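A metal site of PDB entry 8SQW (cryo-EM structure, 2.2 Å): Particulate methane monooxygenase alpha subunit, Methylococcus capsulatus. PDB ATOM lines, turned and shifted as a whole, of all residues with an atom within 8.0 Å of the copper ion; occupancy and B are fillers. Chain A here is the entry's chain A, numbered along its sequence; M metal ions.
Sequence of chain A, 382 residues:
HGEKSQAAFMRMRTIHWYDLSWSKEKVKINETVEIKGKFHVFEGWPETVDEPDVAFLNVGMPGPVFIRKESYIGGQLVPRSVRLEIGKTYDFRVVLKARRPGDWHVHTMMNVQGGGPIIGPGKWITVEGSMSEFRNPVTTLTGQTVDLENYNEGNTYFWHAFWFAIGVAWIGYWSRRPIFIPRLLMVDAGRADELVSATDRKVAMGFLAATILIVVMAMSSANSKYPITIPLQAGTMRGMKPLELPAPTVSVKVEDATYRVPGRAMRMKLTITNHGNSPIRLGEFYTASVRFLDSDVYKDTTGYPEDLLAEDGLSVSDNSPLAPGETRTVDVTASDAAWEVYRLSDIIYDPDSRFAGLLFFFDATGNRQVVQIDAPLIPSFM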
ATOM      1  N   MET A  12     -12.802  37.547   3.578  1.00  0.00           N
ATOM      2  CA  MET A  12     -13.591  36.332   3.682  1.00  0.00           C
ATOM      3  C   MET A  12     -12.960  35.176   2.916  1.00  0.00           C
ATOM      4  O   MET A  12     -12.923  34.047   3.422  1.00  0.00           O
ATOM      5  CB  MET A  12     -15.016  36.575   3.170  1.00  0.00           C
ATOM      6  CG  MET A  12     -15.914  37.311   4.139  1.00  0.00           C
ATOM      7  SD  MET A  12     -17.316  38.082   3.320  1.00  0.00           S
ATOM      8  CE  MET A  12     -18.330  38.512   4.726  1.00  0.00           C
ATOM      9  N   ARG A  13     -12.471  35.421   1.709  1.00  0.00           N
ATOM     10  CA  ARG A  13     -11.920  34.347   0.893  1.00  0.00           C
ATOM     11  C   ARG A  13     -10.435  34.613   0.624  1.00  0.00           C
ATOM     12  O   ARG A  13     -10.040  34.951  -0.496  1.00  0.00           O
ATOM     13  CB  ARG A  13     -12.700  34.259  -0.423  1.00  0.00           C
ATOM     14  CG  ARG A  13     -14.147  34.715  -0.321  1.00  0.00           C
ATOM     15  CD  ARG A  13     -14.656  35.321  -1.624  1.00  0.00           C
ATOM     16  NE  ARG A  13     -14.444  34.446  -2.770  1.00  0.00           N
ATOM     17  CZ  ARG A  13     -15.237  33.436  -3.104  1.00  0.00           C
ATOM     18  NH1 ARG A  13     -16.316  33.144  -2.397  1.00  0.00           N
ATOM     19  NH2 ARG A  13     -14.946  32.715  -4.177  1.00  0.00           N
ATOM     20  N   THR A  14      -9.608  34.438   1.650  1.00  0.00           N
ATOM     21  CA  THR A  14      -8.193  34.171   1.437  1.00  0.00           C
ATOM     22  C   THR A  14      -7.726  32.986   2.267  1.00  0.00           C
ATOM     23  O   THR A  14      -7.292  31.962   1.735  1.00  0.00           O
ATOM     24  CB  THR A  14      -7.355  35.409   1.759  1.00  0.00           C
ATOM     25  OG1 THR A  14      -7.922  36.095   2.869  1.00  0.00           O
ATOM     26  CG2 THR A  14      -7.295  36.332   0.554  1.00  0.00           C
ATOM     27  N   ILE A  15      -7.887  33.112   3.575  1.00  0.00           N
ATOM     28  CA  ILE A  15      -7.323  32.184   4.558  1.00  0.00           C
ATOM     29  C   ILE A  15      -8.225  32.190   5.774  1.00  0.00           C
ATOM     30  O   ILE A  15      -8.529  33.257   6.319  1.00  0.00           O
ATOM     31  CB  ILE A  15      -5.886  32.555   4.956  1.00  0.00           C
ATOM     32  CG1 ILE A  15      -4.890  32.136   3.868  1.00  0.00           C
ATOM     33  CG2 ILE A  15      -5.506  31.934   6.288  1.00  0.00           C
ATOM     34  CD1 ILE A  15      -3.487  32.636   4.115  1.00  0.00           C
ATOM     35  N   HIS A  16      -8.662  31.009   6.203  1.00  0.00           N
ATOM     36  CA  HIS A  16      -9.551  30.883   7.354  1.00  0.00           C
ATOM     37  C   HIS A  16      -8.758  30.348   8.542  1.00  0.00           C
ATOM     38  O   HIS A  16      -8.227  29.236   8.495  1.00  0.00           O
ATOM     39  CB  HIS A  16     -10.723  29.960   7.023  1.00  0.00           C
ATOM     40  CG  HIS A  16     -11.487  30.372   5.811  1.00  0.00           C
ATOM     41  ND1 HIS A  16     -11.981  29.480   4.890  1.00  0.00           N
ATOM     42  CD2 HIS A  16     -11.844  31.609   5.367  1.00  0.00           C
ATOM     43  CE1 HIS A  16     -12.609  30.137   3.935  1.00  0.00           C
ATOM     44  NE2 HIS A  16     -12.545  31.430   4.201  1.00  0.00           N
ATOM     45  N   TRP A  17      -8.676  31.150   9.598  1.00  0.00           N
ATOM     46  CA  TRP A  17      -7.972  30.788  10.818  1.00  0.00           C
ATOM     47  C   TRP A  17      -8.954  30.185  11.808  1.00  0.00           C
ATOM     48  O   TRP A  17     -10.003  30.780  12.078  1.00  0.00           O
ATOM     49  CB  TRP A  17      -7.277  31.999  11.432  1.00  0.00           C
ATOM     50  CG  TRP A  17      -6.483  32.826  10.469  1.00  0.00           C
ATOM     51  CD1 TRP A  17      -6.974  33.758   9.609  1.00  0.00           C
ATOM     52  CD2 TRP A  17      -5.068  32.813  10.296  1.00  0.00           C
ATOM     53  NE1 TRP A  17      -5.944  34.317   8.889  1.00  0.00           N
ATOM     54  CE2 TRP A  17      -4.764  33.757   9.294  1.00  0.00           C
ATOM     55  CE3 TRP A  17      -4.021  32.087  10.876  1.00  0.00           C
ATOM     56  CZ2 TRP A  17      -3.460  33.991   8.863  1.00  0.00           C
ATOM     57  CZ3 TRP A  17      -2.736  32.327  10.442  1.00  0.00           C
ATOM     58  CH2 TRP A  17      -2.465  33.276   9.447  1.00  0.00           C
ATOM     59  N   TYR A  18      -8.617  29.016  12.352  1.00  0.00           N
ATOM     60  CA  TYR A  18      -9.461  28.386  13.362  1.00  0.00           C
ATOM     61  C   TYR A  18      -8.588  27.530  14.263  1.00  0.00           C
ATOM     62  O   TYR A  18      -7.403  27.312  13.993  1.00  0.00           O
ATOM     63  CB  TYR A  18     -10.592  27.562  12.725  1.00  0.00           C
ATOM     64  CG  TYR A  18     -10.135  26.356  11.943  1.00  0.00           C
ATOM     65  CD1 TYR A  18      -9.648  26.481  10.656  1.00  0.00           C
ATOM     66  CD2 TYR A  18     -10.218  25.085  12.488  1.00  0.00           C
ATOM     67  CE1 TYR A  18      -9.245  25.378   9.938  1.00  0.00           C
ATOM     68  CE2 TYR A  18      -9.819  23.977  11.782  1.00  0.00           C
ATOM     69  CZ  TYR A  18      -9.326  24.126  10.506  1.00  0.00           C
ATOM     70  OH  TYR A  18      -8.923  23.024   9.788  1.00  0.00           O
ATOM     71  N   PHE A  39      -4.732  27.193   9.820  1.00  0.00           N
ATOM     72  CA  PHE A  39      -5.264  28.050   8.771  1.00  0.00           C
ATOM     73  C   PHE A  39      -5.500  27.217   7.522  1.00  0.00           C
ATOM     74  O   PHE A  39      -4.699  26.323   7.191  1.00  0.00           O
ATOM     75  CB  PHE A  39      -4.345  29.242   8.470  1.00  0.00           C
ATOM     76  CG  PHE A  39      -2.990  28.860   7.943  1.00  0.00           C
ATOM     77  CD1 PHE A  39      -2.755  28.728   6.578  1.00  0.00           C
ATOM     78  CD2 PHE A  39      -1.920  28.678   8.816  1.00  0.00           C
ATOM     79  CE1 PHE A  39      -1.514  28.389   6.101  1.00  0.00           C
ATOM     80  CE2 PHE A  39      -0.666  28.344   8.338  1.00  0.00           C
ATOM     81  CZ  PHE A  39      -0.470  28.195   6.976  1.00  0.00           C
ATOM     82  N   HIS A  40      -6.599  27.488   6.827  1.00  0.00           N
ATOM     83  CA  HIS A  40      -6.965  26.799   5.608  1.00  0.00           C
ATOM     84  C   HIS A  40      -6.914  27.789   4.451  1.00  0.00           C
ATOM     85  O   HIS A  40      -7.505  28.865   4.519  1.00  0.00           O
ATOM     86  CB  HIS A  40      -8.361  26.191   5.728  1.00  0.00           C
ATOM     87  CG  HIS A  40      -8.872  25.607   4.446  1.00  0.00           C
ATOM     88  ND1 HIS A  40      -9.963  26.113   3.778  1.00  0.00           N
ATOM     89  CD2 HIS A  40      -8.434  24.559   3.698  1.00  0.00           C
ATOM     90  CE1 HIS A  40     -10.177  25.408   2.684  1.00  0.00           C
ATOM     91  NE2 HIS A  40      -9.268  24.455   2.622  1.00  0.00           N
ATOM     92  N   VAL A  41      -6.199  27.414   3.390  1.00  0.00           N
ATOM     93  CA  VAL A  41      -6.108  28.250   2.200  1.00  0.00           C
ATOM     94  C   VAL A  41      -7.349  27.996   1.348  1.00  0.00           C
ATOM     95  O   VAL A  41      -7.586  26.875   0.894  1.00  0.00           O
ATOM     96  CB  VAL A  41      -4.829  27.963   1.414  1.00  0.00           C
ATOM     97  CG1 VAL A  41      -4.640  28.985   0.308  1.00  0.00           C
ATOM     98  CG2 VAL A  41      -3.631  27.946   2.349  1.00  0.00           C
ATOM     99  N   PHE A  42      -8.149  29.042   1.133  1.00  0.00           N
ATOM    100  CA  PHE A  42      -9.425  28.889   0.455  1.00  0.00           C
ATOM    101  C   PHE A  42      -9.221  28.505  -1.007  1.00  0.00           C
ATOM    102  O   PHE A  42      -8.331  29.021  -1.688  1.00  0.00           O
ATOM    103  CB  PHE A  42     -10.226  30.186   0.549  1.00  0.00           C
ATOM    104  CG  PHE A  42     -11.583  30.108  -0.079  1.00  0.00           C
ATOM    105  CD1 PHE A  42     -12.450  29.086   0.244  1.00  0.00           C
ATOM    106  CD2 PHE A  42     -11.983  31.045  -1.010  1.00  0.00           C
ATOM    107  CE1 PHE A  42     -13.701  29.006  -0.332  1.00  0.00           C
ATOM    108  CE2 PHE A  42     -13.240  30.981  -1.582  1.00  0.00           C
ATOM    109  CZ  PHE A  42     -14.089  29.956  -1.246  1.00  0.00           C
ATOM    110  N   GLU A  43     -10.070  27.585  -1.500  1.00  0.00           N
ATOM    111  CA  GLU A  43      -9.959  27.135  -2.877  1.00  0.00           C
ATOM    112  C   GLU A  43     -10.266  28.254  -3.863  1.00  0.00           C
ATOM    113  O   GLU A  43      -9.596  28.374  -4.898  1.00  0.00           O
ATOM    114  CB  GLU A  43     -10.901  25.956  -3.122  1.00  0.00           C
ATOM    115  CG  GLU A  43     -10.419  24.649  -2.512  1.00  0.00           C
ATOM    116  CD  GLU A  43     -10.796  24.506  -1.058  1.00  0.00           C
ATOM    117  OE1 GLU A  43     -11.392  25.448  -0.495  1.00  0.00           O
ATOM    118  OE2 GLU A  43     -10.499  23.442  -0.461  1.00  0.00           O
ATOM    119  N   GLY A  44     -11.266  29.080  -3.563  1.00  0.00           N
ATOM    120  CA  GLY A  44     -11.598  30.196  -4.431  1.00  0.00           C
ATOM    121  C   GLY A  44     -10.712  31.397  -4.188  1.00  0.00           C
ATOM    122  O   GLY A  44     -11.199  32.511  -3.933  1.00  0.00           O
ATOM    123  N   GLY A  87      -6.234  25.194  -0.993  1.00  0.00           N
ATOM    124  CA  GLY A  87      -7.107  24.122  -0.564  1.00  0.00           C
ATOM    125  C   GLY A  87      -6.563  23.296   0.582  1.00  0.00           C
ATOM    126  O   GLY A  87      -7.304  22.458   1.111  1.00  0.00           O
ATOM    127  N   LYS A  88      -5.310  23.502   0.978  1.00  0.00           N
ATOM    128  CA  LYS A  88      -4.712  22.730   2.052  1.00  0.00           C
ATOM    129  C   LYS A  88      -4.878  23.439   3.386  1.00  0.00           C
ATOM    130  O   LYS A  88      -4.969  24.668   3.462  1.00  0.00           O
ATOM    131  CB  LYS A  88      -3.230  22.486   1.760  1.00  0.00           C
ATOM    132  CG  LYS A  88      -2.958  21.557   0.596  1.00  0.00           C
ATOM    133  CD  LYS A  88      -3.323  20.124   0.947  1.00  0.00           C
ATOM    134  CE  LYS A  88      -3.568  19.294  -0.304  1.00  0.00           C
ATOM    135  NZ  LYS A  88      -3.587  17.837  -0.006  1.00  0.00           N
ATOM    136  N   THR A  89      -4.908  22.644   4.446  1.00  0.00           N
ATOM    137  CA  THR A  89      -4.966  23.151   5.815  1.00  0.00           C
ATOM    138  C   THR A  89      -3.634  22.891   6.489  1.00  0.00           C
ATOM    139  O   THR A  89      -3.119  21.764   6.447  1.00  0.00           O
ATOM    140  CB  THR A  89      -6.089  22.485   6.604  1.00  0.00           C
ATOM    141  OG1 THR A  89      -7.340  22.704   5.940  1.00  0.00           O
ATOM    142  CG2 THR A  89      -6.165  23.058   8.010  1.00  0.00           C
ATOM    143  N   TYR A 286     -17.869  30.677  10.904  1.00  0.00           N
ATOM    144  CA  TYR A 286     -16.721  31.586  10.862  1.00  0.00           C
ATOM    145  C   TYR A 286     -16.610  32.112   9.441  1.00  0.00           C
ATOM    146  O   TYR A 286     -16.526  31.326   8.488  1.00  0.00           O
ATOM    147  CB  TYR A 286     -15.454  30.850  11.290  1.00  0.00           C
ATOM    148  CG  TYR A 286     -14.138  31.539  10.959  1.00  0.00           C
ATOM    149  CD1 TYR A 286     -13.562  31.434   9.704  1.00  0.00           C
ATOM    150  CD2 TYR A 286     -13.472  32.264  11.926  1.00  0.00           C
ATOM    151  CE1 TYR A 286     -12.373  32.049   9.405  1.00  0.00           C
ATOM    152  CE2 TYR A 286     -12.276  32.883  11.647  1.00  0.00           C
ATOM    153  CZ  TYR A 286     -11.721  32.772  10.383  1.00  0.00           C
ATOM    154  OH  TYR A 286     -10.530  33.399  10.089  1.00  0.00           O
ATOM    155  N   THR A 287     -16.611  33.434   9.281  1.00  0.00           N
ATOM    156  CA  THR A 287     -16.585  34.053   7.957  1.00  0.00           C
ATOM    157  C   THR A 287     -15.279  34.799   7.711  1.00  0.00           C
ATOM    158  O   THR A 287     -14.568  34.477   6.758  1.00  0.00           O
ATOM    159  CB  THR A 287     -17.799  34.967   7.764  1.00  0.00           C
ATOM    160  OG1 THR A 287     -17.617  35.759   6.587  1.00  0.00           O
ATOM    161  CG2 THR A 287     -18.041  35.853   8.969  1.00  0.00           C
ATOM    162  N   ALA A 356     -17.110  33.590   1.738  1.00  0.00           N
ATOM    163  CA  ALA A 356     -16.691  32.241   2.069  1.00  0.00           C
ATOM    164  C   ALA A 356     -16.561  32.139   3.575  1.00  0.00           C
ATOM    165  O   ALA A 356     -16.357  33.142   4.258  1.00  0.00           O
ATOM    166  CB  ALA A 356     -15.378  31.864   1.386  1.00  0.00           C
ATOM    167  N   GLY A 357     -16.671  30.919   4.075  1.00  0.00           N
ATOM    168  CA  GLY A 357     -16.578  30.726   5.508  1.00  0.00           C
ATOM    169  C   GLY A 357     -16.452  29.255   5.866  1.00  0.00           C
ATOM    170  O   GLY A 357     -16.343  28.395   4.986  1.00  0.00           O
ATOM    171  N   LEU A 358     -16.460  28.992   7.157  1.00  0.00           N
ATOM    172  CA  LEU A 358     -16.384  27.641   7.690  1.00  0.00           C
ATOM    173  C   LEU A 358     -17.577  27.390   8.600  1.00  0.00           C
ATOM    174  O   LEU A 358     -17.903  28.225   9.452  1.00  0.00           O
ATOM    175  CB  LEU A 358     -15.095  27.414   8.467  1.00  0.00           C
ATOM    176  CG  LEU A 358     -13.771  27.579   7.720  1.00  0.00           C
ATOM    177  CD1 LEU A 358     -12.606  27.343   8.675  1.00  0.00           C
ATOM    178  CD2 LEU A 358     -13.702  26.635   6.536  1.00  0.00           C
ATOM    179  N   VAL A 370     -15.712  20.127  10.151  1.00  0.00           N
ATOM    180  CA  VAL A 370     -15.498  21.414   9.514  1.00  0.00           C
ATOM    181  C   VAL A 370     -15.873  21.288   8.048  1.00  0.00           C
ATOM    182  O   VAL A 370     -15.300  20.468   7.326  1.00  0.00           O
ATOM    183  CB  VAL A 370     -14.039  21.891   9.666  1.00  0.00           C
ATOM    184  CG1 VAL A 370     -13.898  23.317   9.140  1.00  0.00           C
ATOM    185  CG2 VAL A 370     -13.599  21.811  11.110  1.00  0.00           C
ATOM    186  N   VAL A 371     -16.821  22.106   7.610  1.00  0.00           N
ATOM    187  CA  VAL A 371     -17.211  22.169   6.208  1.00  0.00           C
ATOM    188  C   VAL A 371     -17.091  23.607   5.752  1.00  0.00           C
ATOM    189  O   VAL A 371     -17.320  24.552   6.513  1.00  0.00           O
ATOM    190  CB  VAL A 371     -18.631  21.614   5.950  1.00  0.00           C
ATOM    191  CG1 VAL A 371     -18.843  20.319   6.720  1.00  0.00           C
ATOM    192  CG2 VAL A 371     -19.690  22.624   6.312  1.00  0.00           C
ATOM    193  N   GLN A 372     -16.691  23.778   4.493  1.00  0.00           N
ATOM    194  CA  GLN A 372     -16.451  25.090   3.923  1.00  0.00           C
ATOM    195  C   GLN A 372     -17.587  25.436   2.958  1.00  0.00           C
ATOM    196  O   GLN A 372     -18.014  24.597   2.161  1.00  0.00           O
ATOM    197  CB  GLN A 372     -15.117  25.133   3.192  1.00  0.00           C
ATOM    198  CG  GLN A 372     -14.822  26.434   2.500  1.00  0.00           C
ATOM    199  CD  GLN A 372     -13.370  26.573   2.129  1.00  0.00           C
ATOM    200  OE1 GLN A 372     -12.602  27.259   2.796  1.00  0.00           O
ATOM    201  NE2 GLN A 372     -12.977  25.918   1.037  1.00  0.00           N
ATOM    202  N   ILE A 373     -18.075  26.672   3.045  1.00  0.00           N
ATOM    203  CA  ILE A 373     -19.159  27.156   2.202  1.00  0.00           C
ATOM    204  C   ILE A 373     -18.723  28.445   1.537  1.00  0.00           C
ATOM    205  O   ILE A 373     -17.985  29.250   2.121  1.00  0.00           O
ATOM    206  CB  ILE A 373     -20.456  27.365   3.007  1.00  0.00           C
ATOM    207  CG1 ILE A 373     -20.202  28.285   4.202  1.00  0.00           C
ATOM    208  CG2 ILE A 373     -21.034  26.035   3.464  1.00  0.00           C
ATOM    209  CD1 ILE A 373     -21.457  28.835   4.831  1.00  0.00           C
HETATM  210 CU    CU M   1     -10.745  28.004   4.111  1.00  0.00          CU
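Merely in contact with the copper ion: Phe 42 (3.99 Å).
A ring nitrogen (NE2) of His 40 sits at hydrogen-bond distance from the side-chain carboxylate (OE2) of Glu 43 (3.5 Å).
NE2 of His 40 sits at hydrogen-bond distance from O of Gly 87.
O of Met 12 lies within hydrogen-bond range of NE2 of His 16 (2.8 Å).
The backbone carbonyl oxygen (O) of Thr 14 is in hydrogen-bond range of the backbone NH (N) of Phe 42 (3.1 Å).
The copper ion is bound by ND1 of His 40 (2.1 Å), ND1 of His 16 (2.1 Å) and OE1 of Gln 372 (2.4 Å).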
